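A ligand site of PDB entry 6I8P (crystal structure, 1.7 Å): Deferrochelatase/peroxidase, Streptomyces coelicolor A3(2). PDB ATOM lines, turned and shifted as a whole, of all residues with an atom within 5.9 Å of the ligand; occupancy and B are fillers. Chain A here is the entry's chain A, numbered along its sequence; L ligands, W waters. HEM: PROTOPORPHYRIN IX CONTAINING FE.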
ATOM      1  N   ASN A 179      34.979 -18.716   9.568  1.00  0.00           N
ATOM      2  CA  ASN A 179      34.779 -19.204  10.924  1.00  0.00           C
ATOM      3  C   ASN A 179      34.876 -20.741  10.940  1.00  0.00           C
ATOM      4  O   ASN A 179      35.154 -21.382   9.911  1.00  0.00           O
ATOM      5  CB  ASN A 179      33.455 -18.674  11.485  1.00  0.00           C
ATOM      6  CG  ASN A 179      32.275 -18.979  10.581  1.00  0.00           C
ATOM      7  OD1 ASN A 179      32.093 -20.124  10.159  1.00  0.00           O
ATOM      8  ND2 ASN A 179      31.459 -17.977  10.279  1.00  0.00           N
ATOM      9  N   LEU A 181      32.638 -22.901  11.060  1.00  0.00           N
ATOM     10  CA  LEU A 181      31.605 -23.559  10.281  1.00  0.00           C
ATOM     11  C   LEU A 181      31.933 -23.605   8.799  1.00  0.00           C
ATOM     12  O   LEU A 181      31.146 -24.145   8.025  1.00  0.00           O
ATOM     13  CB  LEU A 181      30.256 -22.849  10.471  1.00  0.00           C
ATOM     14  CG  LEU A 181      29.784 -22.814  11.917  1.00  0.00           C
ATOM     15  CD1 LEU A 181      28.391 -22.196  12.017  1.00  0.00           C
ATOM     16  CD2 LEU A 181      29.819 -24.218  12.484  1.00  0.00           C
ATOM     17  N   PHE A 183      32.345 -20.975   6.691  1.00  0.00           N
ATOM     18  CA  PHE A 183      31.822 -19.864   5.914  1.00  0.00           C
ATOM     19  C   PHE A 183      32.649 -18.596   6.131  1.00  0.00           C
ATOM     20  O   PHE A 183      33.124 -18.321   7.241  1.00  0.00           O
ATOM     21  CB  PHE A 183      30.362 -19.578   6.281  1.00  0.00           C
ATOM     22  CG  PHE A 183      29.395 -20.457   5.582  1.00  0.00           C
ATOM     23  CD1 PHE A 183      29.181 -21.776   6.002  1.00  0.00           C
ATOM     24  CD2 PHE A 183      28.673 -19.992   4.495  1.00  0.00           C
ATOM     25  CE1 PHE A 183      28.275 -22.604   5.330  1.00  0.00           C
ATOM     26  CE2 PHE A 183      27.765 -20.809   3.843  1.00  0.00           C
ATOM     27  CZ  PHE A 183      27.586 -22.126   4.255  1.00  0.00           C
ATOM     28  N   LYS A 184      32.784 -17.815   5.057  1.00  0.00           N
ATOM     29  CA  LYS A 184      33.381 -16.483   5.200  1.00  0.00           C
ATOM     30  C   LYS A 184      32.557 -15.657   6.178  1.00  0.00           C
ATOM     31  O   LYS A 184      31.328 -15.687   6.177  1.00  0.00           O
ATOM     32  CB  LYS A 184      33.438 -15.788   3.839  1.00  0.00           C
ATOM     33  CG  LYS A 184      34.447 -16.373   2.861  1.00  0.00           C
ATOM     34  CD  LYS A 184      34.281 -15.730   1.475  1.00  0.00           C
ATOM     35  CE  LYS A 184      35.352 -16.171   0.502  1.00  0.00           C
ATOM     36  NZ  LYS A 184      35.023 -15.670  -0.866  1.00  0.00           N
ATOM     37  N   ASP A 185      33.244 -14.929   7.047  1.00  0.00           N
ATOM     38  CA  ASP A 185      32.587 -14.141   8.088  1.00  0.00           C
ATOM     39  C   ASP A 185      33.193 -12.748   8.054  1.00  0.00           C
ATOM     40  O   ASP A 185      34.379 -12.593   8.355  1.00  0.00           O
ATOM     41  CB  ASP A 185      32.797 -14.783   9.468  1.00  0.00           C
ATOM     42  CG  ASP A 185      31.653 -14.520  10.448  1.00  0.00           C
ATOM     43  OD1 ASP A 185      30.935 -13.484  10.338  1.00  0.00           O
ATOM     44  OD2 ASP A 185      31.492 -15.371  11.337  1.00  0.00           O
ATOM     45  N   GLY A 186      32.392 -11.741   7.697  1.00  0.00           N
ATOM     46  CA  GLY A 186      32.871 -10.362   7.726  1.00  0.00           C
ATOM     47  C   GLY A 186      32.634  -9.568   6.447  1.00  0.00           C
ATOM     48  O   GLY A 186      32.974  -8.386   6.384  1.00  0.00           O
ATOM     49  N   THR A 187      32.010 -10.195   5.443  1.00  0.00           N
ATOM     50  CA  THR A 187      31.818  -9.574   4.136  1.00  0.00           C
ATOM     51  C   THR A 187      31.123  -8.211   4.255  1.00  0.00           C
ATOM     52  O   THR A 187      31.661  -7.184   3.835  1.00  0.00           O
ATOM     53  CB  THR A 187      31.013 -10.522   3.234  1.00  0.00           C
ATOM     54  OG1 THR A 187      31.680 -11.794   3.197  1.00  0.00           O
ATOM     55  CG2 THR A 187      30.884  -9.976   1.806  1.00  0.00           C
ATOM     56  N   ARG A 188      29.915  -8.184   4.813  1.00  0.00           N
ATOM     57  CA  ARG A 188      29.167  -6.932   4.932  1.00  0.00           C
ATOM     58  C   ARG A 188      29.281  -6.424   6.366  1.00  0.00           C
ATOM     59  O   ARG A 188      28.366  -6.522   7.184  1.00  0.00           O
ATOM     60  CB  ARG A 188      27.722  -7.138   4.497  1.00  0.00           C
ATOM     61  CG  ARG A 188      27.539  -7.061   2.973  1.00  0.00           C
ATOM     62  CD  ARG A 188      26.070  -7.164   2.538  1.00  0.00           C
ATOM     63  NE  ARG A 188      25.237  -6.505   3.534  1.00  0.00           N
ATOM     64  CZ  ARG A 188      25.000  -5.203   3.555  1.00  0.00           C
ATOM     65  NH1 ARG A 188      24.252  -4.692   4.520  1.00  0.00           N
ATOM     66  NH2 ARG A 188      25.492  -4.408   2.607  1.00  0.00           N
ATOM     67  N   ASN A 189      30.447  -5.901   6.653  1.00  0.00           N
ATOM     68  CA  ASN A 189      30.729  -5.253   7.925  1.00  0.00           C
ATOM     69  C   ASN A 189      30.874  -3.762   7.667  1.00  0.00           C
ATOM     70  O   ASN A 189      30.557  -3.274   6.575  1.00  0.00           O
ATOM     71  CB  ASN A 189      31.972  -5.878   8.563  1.00  0.00           C
ATOM     72  CG  ASN A 189      31.980  -5.734  10.050  1.00  0.00           C
ATOM     73  OD1 ASN A 189      30.932  -5.684  10.675  1.00  0.00           O
ATOM     74  ND2 ASN A 189      33.179  -5.652  10.636  1.00  0.00           N
ATOM     75  N   ILE A 224      29.956 -17.927  22.157  1.00  0.00           N
ATOM     76  CA  ILE A 224      28.964 -18.758  21.481  1.00  0.00           C
ATOM     77  C   ILE A 224      29.583 -20.109  21.176  1.00  0.00           C
ATOM     78  O   ILE A 224      30.547 -20.206  20.409  1.00  0.00           O
ATOM     79  CB  ILE A 224      28.467 -18.100  20.191  1.00  0.00           C
ATOM     80  CG1 ILE A 224      28.069 -16.646  20.505  1.00  0.00           C
ATOM     81  CG2 ILE A 224      27.310 -18.909  19.601  1.00  0.00           C
ATOM     82  CD1 ILE A 224      27.722 -15.812  19.283  1.00  0.00           C
ATOM     83  N   MET A 226      29.576 -23.705  19.348  1.00  0.00           N
ATOM     84  CA  MET A 226      29.076 -24.297  18.109  1.00  0.00           C
ATOM     85  C   MET A 226      28.922 -25.811  18.251  1.00  0.00           C
ATOM     86  O   MET A 226      29.833 -26.490  18.747  1.00  0.00           O
ATOM     87  CB  MET A 226      30.018 -24.004  16.943  1.00  0.00           C
ATOM     88  CG  MET A 226      30.179 -22.521  16.661  1.00  0.00           C
ATOM     89  SD  MET A 226      31.593 -22.285  15.554  1.00  0.00           S
ATOM     90  CE  MET A 226      31.150 -20.734  14.824  1.00  0.00           C
ATOM     91  N   PHE A 243      22.488 -19.943   6.011  1.00  0.00           N
ATOM     92  CA  PHE A 243      23.086 -18.618   5.935  1.00  0.00           C
ATOM     93  C   PHE A 243      22.471 -17.725   4.860  1.00  0.00           C
ATOM     94  O   PHE A 243      22.283 -16.514   5.089  1.00  0.00           O
ATOM     95  CB  PHE A 243      24.594 -18.748   5.721  1.00  0.00           C
ATOM     96  CG  PHE A 243      25.327 -19.071   7.000  1.00  0.00           C
ATOM     97  CD1 PHE A 243      25.306 -18.172   8.063  1.00  0.00           C
ATOM     98  CD2 PHE A 243      25.985 -20.284   7.148  1.00  0.00           C
ATOM     99  CE1 PHE A 243      25.946 -18.473   9.274  1.00  0.00           C
ATOM    100  CE2 PHE A 243      26.624 -20.593   8.353  1.00  0.00           C
ATOM    101  CZ  PHE A 243      26.606 -19.680   9.415  1.00  0.00           C
ATOM    102  N   ARG A 245      24.099 -17.637   1.860  1.00  0.00           N
ATOM    103  CA  ARG A 245      25.224 -17.508   0.966  1.00  0.00           C
ATOM    104  C   ARG A 245      25.741 -18.908   0.669  1.00  0.00           C
ATOM    105  O   ARG A 245      25.572 -19.824   1.479  1.00  0.00           O
ATOM    106  CB  ARG A 245      26.351 -16.644   1.569  1.00  0.00           C
ATOM    107  CG  ARG A 245      25.988 -15.163   1.732  1.00  0.00           C
ATOM    108  CD  ARG A 245      27.094 -14.385   2.448  1.00  0.00           C
ATOM    109  NE  ARG A 245      26.792 -12.970   2.591  1.00  0.00           N
ATOM    110  CZ  ARG A 245      27.115 -12.034   1.708  1.00  0.00           C
ATOM    111  NH1 ARG A 245      27.752 -12.356   0.593  1.00  0.00           N
ATOM    112  NH2 ARG A 245      26.804 -10.764   1.938  1.00  0.00           N
ATOM    113  N   PRO A 262      23.239  -8.758  -1.457  1.00  0.00           N
ATOM    114  CA  PRO A 262      22.240  -9.815  -1.277  1.00  0.00           C
ATOM    115  C   PRO A 262      20.879  -9.379  -1.792  1.00  0.00           C
ATOM    116  O   PRO A 262      20.531  -8.200  -1.767  1.00  0.00           O
ATOM    117  CB  PRO A 262      22.222 -10.039   0.243  1.00  0.00           C
ATOM    118  CG  PRO A 262      22.890  -8.850   0.820  1.00  0.00           C
ATOM    119  CD  PRO A 262      23.818  -8.286  -0.203  1.00  0.00           C
ATOM    120  N   HIS A 272      20.067 -16.672   8.173  1.00  0.00           N
ATOM    121  CA  HIS A 272      20.789 -15.787   9.082  1.00  0.00           C
ATOM    122  C   HIS A 272      21.003 -14.403   8.483  1.00  0.00           C
ATOM    123  O   HIS A 272      20.736 -13.396   9.125  1.00  0.00           O
ATOM    124  CB  HIS A 272      22.121 -16.422   9.448  1.00  0.00           C
ATOM    125  CG  HIS A 272      22.919 -15.620  10.423  1.00  0.00           C
ATOM    126  ND1 HIS A 272      22.596 -15.567  11.767  1.00  0.00           N
ATOM    127  CD2 HIS A 272      24.029 -14.863  10.272  1.00  0.00           C
ATOM    128  CE1 HIS A 272      23.475 -14.803  12.392  1.00  0.00           C
ATOM    129  NE2 HIS A 272      24.354 -14.366  11.504  1.00  0.00           N
ATOM    130  N   VAL A 273      21.503 -14.345   7.240  1.00  0.00           N
ATOM    131  CA  VAL A 273      21.804 -13.067   6.604  1.00  0.00           C
ATOM    132  C   VAL A 273      20.523 -12.270   6.383  1.00  0.00           C
ATOM    133  O   VAL A 273      20.503 -11.050   6.552  1.00  0.00           O
ATOM    134  CB  VAL A 273      22.565 -13.290   5.287  1.00  0.00           C
ATOM    135  CG1 VAL A 273      22.570 -12.019   4.464  1.00  0.00           C
ATOM    136  CG2 VAL A 273      23.964 -13.735   5.599  1.00  0.00           C
ATOM    137  N   ALA A 276      19.586 -10.856   9.883  1.00  0.00           N
ATOM    138  CA  ALA A 276      20.558  -9.945  10.475  1.00  0.00           C
ATOM    139  C   ALA A 276      20.741  -8.660   9.681  1.00  0.00           C
ATOM    140  O   ALA A 276      21.298  -7.688  10.204  1.00  0.00           O
ATOM    141  CB  ALA A 276      21.920 -10.621  10.598  1.00  0.00           C
ATOM    142  N   HIS A 277      20.298  -8.655   8.422  1.00  0.00           N
ATOM    143  CA  HIS A 277      20.605  -7.577   7.505  1.00  0.00           C
ATOM    144  C   HIS A 277      19.997  -6.277   8.004  1.00  0.00           C
ATOM    145  O   HIS A 277      18.872  -6.275   8.504  1.00  0.00           O
ATOM    146  CB  HIS A 277      20.066  -7.919   6.113  1.00  0.00           C
ATOM    147  CG  HIS A 277      20.522  -7.000   5.027  1.00  0.00           C
ATOM    148  ND1 HIS A 277      19.935  -5.772   4.789  1.00  0.00           N
ATOM    149  CD2 HIS A 277      21.488  -7.138   4.084  1.00  0.00           C
ATOM    150  CE1 HIS A 277      20.535  -5.188   3.773  1.00  0.00           C
ATOM    151  NE2 HIS A 277      21.475  -5.990   3.322  1.00  0.00           N
ATOM    152  N   PRO A 278      20.725  -5.159   7.902  1.00  0.00           N
ATOM    153  CA  PRO A 278      20.147  -3.874   8.352  1.00  0.00           C
ATOM    154  C   PRO A 278      18.754  -3.617   7.808  1.00  0.00           C
ATOM    155  O   PRO A 278      17.905  -3.076   8.534  1.00  0.00           O
ATOM    156  CB  PRO A 278      21.167  -2.844   7.814  1.00  0.00           C
ATOM    157  CG  PRO A 278      22.464  -3.569   7.763  1.00  0.00           C
ATOM    158  CD  PRO A 278      22.152  -5.045   7.565  1.00  0.00           C
ATOM    159  N   LEU A 286      25.990  -2.976  12.737  1.00  0.00           N
ATOM    160  CA  LEU A 286      26.964  -3.332  13.757  1.00  0.00           C
ATOM    161  C   LEU A 286      28.345  -3.373  13.135  1.00  0.00           C
ATOM    162  O   LEU A 286      28.491  -3.647  11.944  1.00  0.00           O
ATOM    163  CB  LEU A 286      26.652  -4.707  14.370  1.00  0.00           C
ATOM    164  CG  LEU A 286      25.308  -4.811  15.060  1.00  0.00           C
ATOM    165  CD1 LEU A 286      25.050  -6.248  15.519  1.00  0.00           C
ATOM    166  CD2 LEU A 286      25.275  -3.817  16.229  1.00  0.00           C
ATOM    167  N   ARG A 288      31.208  -5.791  13.541  1.00  0.00           N
ATOM    168  CA  ARG A 288      31.542  -7.095  14.097  1.00  0.00           C
ATOM    169  C   ARG A 288      33.057  -7.277  14.128  1.00  0.00           C
ATOM    170  O   ARG A 288      33.742  -6.968  13.146  1.00  0.00           O
ATOM    171  CB  ARG A 288      30.883  -8.207  13.275  1.00  0.00           C
ATOM    172  CG  ARG A 288      29.377  -8.363  13.544  1.00  0.00           C
ATOM    173  CD  ARG A 288      28.726  -9.321  12.574  1.00  0.00           C
ATOM    174  NE  ARG A 288      28.786  -8.804  11.213  1.00  0.00           N
ATOM    175  CZ  ARG A 288      29.123  -9.512  10.135  1.00  0.00           C
ATOM    176  NH1 ARG A 288      29.438 -10.803  10.238  1.00  0.00           N
ATOM    177  NH2 ARG A 288      29.139  -8.913   8.949  1.00  0.00           N
ATOM    178  N   LEU A 307      32.728 -19.408  18.816  1.00  0.00           N
ATOM    179  CA  LEU A 307      33.034 -18.082  18.298  1.00  0.00           C
ATOM    180  C   LEU A 307      32.851 -17.090  19.421  1.00  0.00           C
ATOM    181  O   LEU A 307      31.820 -17.084  20.101  1.00  0.00           O
ATOM    182  CB  LEU A 307      32.122 -17.731  17.116  1.00  0.00           C
ATOM    183  CG  LEU A 307      32.409 -16.426  16.399  1.00  0.00           C
ATOM    184  CD1 LEU A 307      32.185 -16.615  14.911  1.00  0.00           C
ATOM    185  CD2 LEU A 307      31.503 -15.342  16.944  1.00  0.00           C
ATOM    186  N   PHE A 309      32.094 -13.679  19.989  1.00  0.00           N
ATOM    187  CA  PHE A 309      31.484 -12.625  19.195  1.00  0.00           C
ATOM    188  C   PHE A 309      31.620 -11.267  19.902  1.00  0.00           C
ATOM    189  O   PHE A 309      31.314 -11.145  21.091  1.00  0.00           O
ATOM    190  CB  PHE A 309      30.010 -12.982  18.955  1.00  0.00           C
ATOM    191  CG  PHE A 309      29.242 -11.954  18.161  1.00  0.00           C
ATOM    192  CD1 PHE A 309      29.159 -12.043  16.774  1.00  0.00           C
ATOM    193  CD2 PHE A 309      28.561 -10.930  18.807  1.00  0.00           C
ATOM    194  CE1 PHE A 309      28.444 -11.085  16.033  1.00  0.00           C
ATOM    195  CE2 PHE A 309      27.836  -9.981  18.094  1.00  0.00           C
ATOM    196  CZ  PHE A 309      27.782 -10.059  16.690  1.00  0.00           C
ATOM    197  N   PHE A 320      22.954  -4.034  18.912  1.00  0.00           N
ATOM    198  CA  PHE A 320      22.886  -5.457  19.190  1.00  0.00           C
ATOM    199  C   PHE A 320      21.476  -5.916  19.543  1.00  0.00           C
ATOM    200  O   PHE A 320      21.029  -6.989  19.104  1.00  0.00           O
ATOM    201  CB  PHE A 320      23.864  -5.818  20.314  1.00  0.00           C
ATOM    202  CG  PHE A 320      23.871  -7.259  20.655  1.00  0.00           C
ATOM    203  CD1 PHE A 320      24.556  -8.180  19.861  1.00  0.00           C
ATOM    204  CD2 PHE A 320      23.167  -7.721  21.752  1.00  0.00           C
ATOM    205  CE1 PHE A 320      24.554  -9.531  20.170  1.00  0.00           C
ATOM    206  CE2 PHE A 320      23.162  -9.078  22.069  1.00  0.00           C
ATOM    207  CZ  PHE A 320      23.851  -9.978  21.280  1.00  0.00           C
ATOM    208  N   VAL A 323      18.924  -6.439  16.589  1.00  0.00           N
ATOM    209  CA  VAL A 323      19.350  -7.507  15.683  1.00  0.00           C
ATOM    210  C   VAL A 323      19.268  -8.862  16.379  1.00  0.00           C
ATOM    211  O   VAL A 323      18.795  -9.851  15.803  1.00  0.00           O
ATOM    212  CB  VAL A 323      20.752  -7.228  15.123  1.00  0.00           C
ATOM    213  CG1 VAL A 323      21.152  -8.340  14.146  1.00  0.00           C
ATOM    214  CG2 VAL A 323      20.816  -5.860  14.429  1.00  0.00           C
ATOM    215  N   GLN A 324      19.712  -8.942  17.636  1.00  0.00           N
ATOM    216  CA  GLN A 324      19.641 -10.243  18.310  1.00  0.00           C
ATOM    217  C   GLN A 324      18.188 -10.665  18.539  1.00  0.00           C
ATOM    218  O   GLN A 324      17.865 -11.853  18.445  1.00  0.00           O
ATOM    219  CB  GLN A 324      20.414 -10.204  19.625  1.00  0.00           C
ATOM    220  CG  GLN A 324      20.401 -11.534  20.412  1.00  0.00           C
ATOM    221  CD  GLN A 324      21.047 -12.728  19.677  1.00  0.00           C
ATOM    222  OE1 GLN A 324      21.932 -12.562  18.842  1.00  0.00           O
ATOM    223  NE2 GLN A 324      20.600 -13.932  20.006  1.00  0.00           N
ATOM    224  N   LEU A 327      16.867 -12.477  15.626  1.00  0.00           N
ATOM    225  CA  LEU A 327      17.415 -13.801  15.374  1.00  0.00           C
ATOM    226  C   LEU A 327      16.724 -14.881  16.202  1.00  0.00           C
ATOM    227  O   LEU A 327      17.208 -16.023  16.229  1.00  0.00           O
ATOM    228  CB  LEU A 327      18.922 -13.821  15.654  1.00  0.00           C
ATOM    229  CG  LEU A 327      19.786 -12.850  14.866  1.00  0.00           C
ATOM    230  CD1 LEU A 327      21.275 -13.079  15.155  1.00  0.00           C
ATOM    231  CD2 LEU A 327      19.487 -12.943  13.361  1.00  0.00           C
ATOM    232  N   LEU A 332      20.202 -20.646  12.244  1.00  0.00           N
ATOM    233  CA  LEU A 332      21.491 -20.938  12.859  1.00  0.00           C
ATOM    234  C   LEU A 332      21.337 -21.365  14.310  1.00  0.00           C
ATOM    235  O   LEU A 332      22.203 -22.055  14.842  1.00  0.00           O
ATOM    236  CB  LEU A 332      22.399 -19.703  12.769  1.00  0.00           C
ATOM    237  CG  LEU A 332      23.804 -19.803  13.356  1.00  0.00           C
ATOM    238  CD1 LEU A 332      24.607 -20.892  12.666  1.00  0.00           C
ATOM    239  CD2 LEU A 332      24.517 -18.452  13.235  1.00  0.00           C
ATOM    240  N   ILE A 336      24.114 -23.459  17.507  1.00  0.00           N
ATOM    241  CA  ILE A 336      24.908 -22.614  18.380  1.00  0.00           C
ATOM    242  C   ILE A 336      24.200 -22.458  19.712  1.00  0.00           C
ATOM    243  O   ILE A 336      23.004 -22.738  19.847  1.00  0.00           O
ATOM    244  CB  ILE A 336      25.171 -21.217  17.775  1.00  0.00           C
ATOM    245  CG1 ILE A 336      23.852 -20.458  17.574  1.00  0.00           C
ATOM    246  CG2 ILE A 336      25.959 -21.335  16.468  1.00  0.00           C
ATOM    247  CD1 ILE A 336      24.025 -18.965  17.586  1.00  0.00           C
ATOM    248  N   HIS A 338      24.540 -19.541  23.150  1.00  0.00           N
ATOM    249  CA  HIS A 338      25.228 -18.433  23.810  1.00  0.00           C
ATOM    250  C   HIS A 338      25.484 -18.806  25.266  1.00  0.00           C
ATOM    251  O   HIS A 338      24.532 -19.056  26.019  1.00  0.00           O
ATOM    252  CB  HIS A 338      24.382 -17.160  23.750  1.00  0.00           C
ATOM    253  CG  HIS A 338      24.238 -16.573  22.386  1.00  0.00           C
ATOM    254  ND1 HIS A 338      24.628 -15.289  22.075  1.00  0.00           N
ATOM    255  CD2 HIS A 338      23.747 -17.101  21.226  1.00  0.00           C
ATOM    256  CE1 HIS A 338      24.383 -15.041  20.811  1.00  0.00           C
ATOM    257  NE2 HIS A 338      23.844 -16.125  20.266  1.00  0.00           N
HETATM  258  CHA HEM L   1      26.601 -12.009   8.587  1.00  0.00           C
HETATM  259  CHB HEM L   1      28.006 -16.195  10.627  1.00  0.00           C
HETATM  260  CHC HEM L   1      26.466 -14.660  14.975  1.00  0.00           C
HETATM  261  CHD HEM L   1      25.069 -10.493  12.925  1.00  0.00           C
HETATM  262  C1A HEM L   1      27.116 -13.271   8.779  1.00  0.00           C
HETATM  263  C2A HEM L   1      27.672 -14.101   7.752  1.00  0.00           C
HETATM  264  C3A HEM L   1      28.036 -15.250   8.319  1.00  0.00           C
HETATM  265  C4A HEM L   1      27.747 -15.179   9.717  1.00  0.00           C
HETATM  266  CMA HEM L   1      28.703 -16.474   7.636  1.00  0.00           C
HETATM  267  CAA HEM L   1      27.763 -13.711   6.258  1.00  0.00           C
HETATM  268  CBA HEM L   1      28.996 -12.905   5.854  1.00  0.00           C
HETATM  269  CGA HEM L   1      29.067 -11.509   6.438  1.00  0.00           C
HETATM  270  O1A HEM L   1      29.793 -11.351   7.445  1.00  0.00           O
HETATM  271  O2A HEM L   1      28.425 -10.570   5.891  1.00  0.00           O
HETATM  272  C1B HEM L   1      27.738 -16.128  11.980  1.00  0.00           C
HETATM  273  C2B HEM L   1      28.080 -17.133  12.950  1.00  0.00           C
HETATM  274  C3B HEM L   1      27.637 -16.722  14.157  1.00  0.00           C
HETATM  275  C4B HEM L   1      27.024 -15.421  13.974  1.00  0.00           C
HETATM  276  CMB HEM L   1      28.805 -18.455  12.596  1.00  0.00           C
HETATM  277  CAB HEM L   1      27.764 -17.427  15.545  1.00  0.00           C
HETATM  278  CBB HEM L   1      28.539 -18.503  15.718  1.00  0.00           C
HETATM  279  C1C HEM L   1      25.932 -13.404  14.809  1.00  0.00           C
HETATM  280  C2C HEM L   1      25.281 -12.605  15.835  1.00  0.00           C
HETATM  281  C3C HEM L   1      24.892 -11.450  15.248  1.00  0.00           C
HETATM  282  C4C HEM L   1      25.285 -11.493  13.853  1.00  0.00           C
HETATM  283  CMC HEM L   1      25.125 -13.059  17.305  1.00  0.00           C
HETATM  284  CAC HEM L   1      24.162 -10.222  15.850  1.00  0.00           C
HETATM  285  CBC HEM L   1      23.587 -10.275  17.062  1.00  0.00           C
HETATM  286  C1D HEM L   1      25.406 -10.527  11.589  1.00  0.00           C
HETATM  287  C2D HEM L   1      25.283  -9.429  10.658  1.00  0.00           C
HETATM  288  C3D HEM L   1      25.698  -9.833   9.443  1.00  0.00           C
HETATM  289  C4D HEM L   1      26.105 -11.223   9.582  1.00  0.00           C
HETATM  290  CMD HEM L   1      24.758  -8.022  10.996  1.00  0.00           C
HETATM  291  CAD HEM L   1      25.723  -8.985   8.167  1.00  0.00           C
HETATM  292  CBD HEM L   1      24.426  -9.175   7.387  1.00  0.00           C
HETATM  293  CGD HEM L   1      24.354  -8.219   6.227  1.00  0.00           C
HETATM  294  O1D HEM L   1      24.460  -8.657   5.054  1.00  0.00           O
HETATM  295  O2D HEM L   1      24.220  -7.006   6.497  1.00  0.00           O
HETATM  296  NA  HEM L   1      27.166 -13.955   9.986  1.00  0.00           N
HETATM  297  NB  HEM L   1      27.098 -15.108  12.628  1.00  0.00           N
HETATM  298  NC  HEM L   1      25.889 -12.705  13.631  1.00  0.00           N
HETATM  299  ND  HEM L   1      25.925 -11.595  10.901  1.00  0.00           N
HETATM  300 FE   HEM L   1      26.389 -13.406  11.766  1.00  0.00          FE
HETATM  301  O   HOH W   1      26.023  -5.288   7.858  1.00  0.00           O
HETATM  302  O   HOH W   2      22.760  -5.445  11.224  1.00  0.00           O
HETATM  303  O   HOH W   3      26.110 -10.920   4.525  1.00  0.00           O
HETATM  304  O   HOH W   4      25.346  -4.874  10.465  1.00  0.00           O
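Water W3 lies within hydrogen-bond range of NH2 of Arg 245 (2.7 Å) and O2A of the ligand (2.7 Å). Water W1 lies within hydrogen-bond range of O of Arg 188 (2.7 Å) and O2D of the ligand (2.8 Å).
A ring nitrogen (NE2) of His 272 is bound to an iron atom (FE) of the ligand. An oxygen (O2A) of the ligand lies within hydrogen-bond range of the backbone NH (N) of Arg 188, 3.0 Å away. An oxygen (O1A) of the ligand is in hydrogen-bond range of the backbone NH (N) of Gly 186. An oxygen (O1A) of the ligand is in hydrogen-bond range of the backbone NH (N) of Thr 187 (3.2 Å). NE of Arg 188 lies within salt-bridge range of O1D of the ligand (2.7 Å). NH1 of Arg 288 lies within salt-bridge range of O1A of the ligand, 2.9 Å away.
Merely in contact with the ligand: Pro 278 (3.0 Å), Lys 184 (3.1 Å), Gln 324 (3.3 Å), Phe 320 (3.3 Å), Phe 243 (3.4 Å), His 277 (3.5 Å), Phe 309 (3.5 Å), Met 226 (3.5 Å), Asn 179 (3.6 Å), Ala 276 (3.6 Å), Asp 185 (3.7 Å), Leu 332 (3.7 Å), Phe 183 (3.8 Å), Leu 181 (3.8 Å), Val 273 (3.9 Å), Arg 245 (3.9 Å), Ile 336 (3.9 Å), Leu 307 (3.9 Å), Val 323 (3.9 Å) and Leu 327 (3.97 Å). Hydrophobic or aromatic side chains that line the ligand: Leu 181, Phe 183, Met 226, Phe 243, His 272, Val 273, Ala 276, His 277, Pro 278, Leu 307, Phe 309, Phe 320, Val 323, Leu 327, Leu 332 and Ile 336. Within 4 Å of the ligand: Asn 179, Leu 181, Phe 183, Lys 184, Asp 185, Gly 186, Thr 187, Arg 188, Met 226, Phe 243, Arg 245, His 272, Val 273, Ala 276, His 277, Pro 278, Arg 288, Leu 307, Phe 309, Phe 320, Val 323, Gln 324, Leu 327, Leu 332 and Ile 336.
The backbone NH of Leu 307 is in hydrogen-bond range of the backbone carbonyl oxygen of Ile 224, at 2.8 Å. The side-chain carboxylate (OD1) of Asp 185 is in salt-bridge range of the guanidinium group (NH1) of Arg 288 (3.1 Å). N of Arg 288 sits at hydrogen-bond distance from OD1 of Asn 189. N of Leu 181 lies within hydrogen-bond range of OD1 of Asn 179 (3.0 Å). OD2 of Asp 185 sits at hydrogen-bond distance from ND2 of Asn 179 (2.8 Å). N of Val 273 sits at hydrogen-bond distance from O of Phe 243 (3.2 Å). The side-chain amide nitrogen of Asn 179 lies within hydrogen-bond range of the backbone carbonyl oxygen of Phe 183. O of Arg 188 sits at hydrogen-bond distance from NH2 of Arg 288 (3.1 Å).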
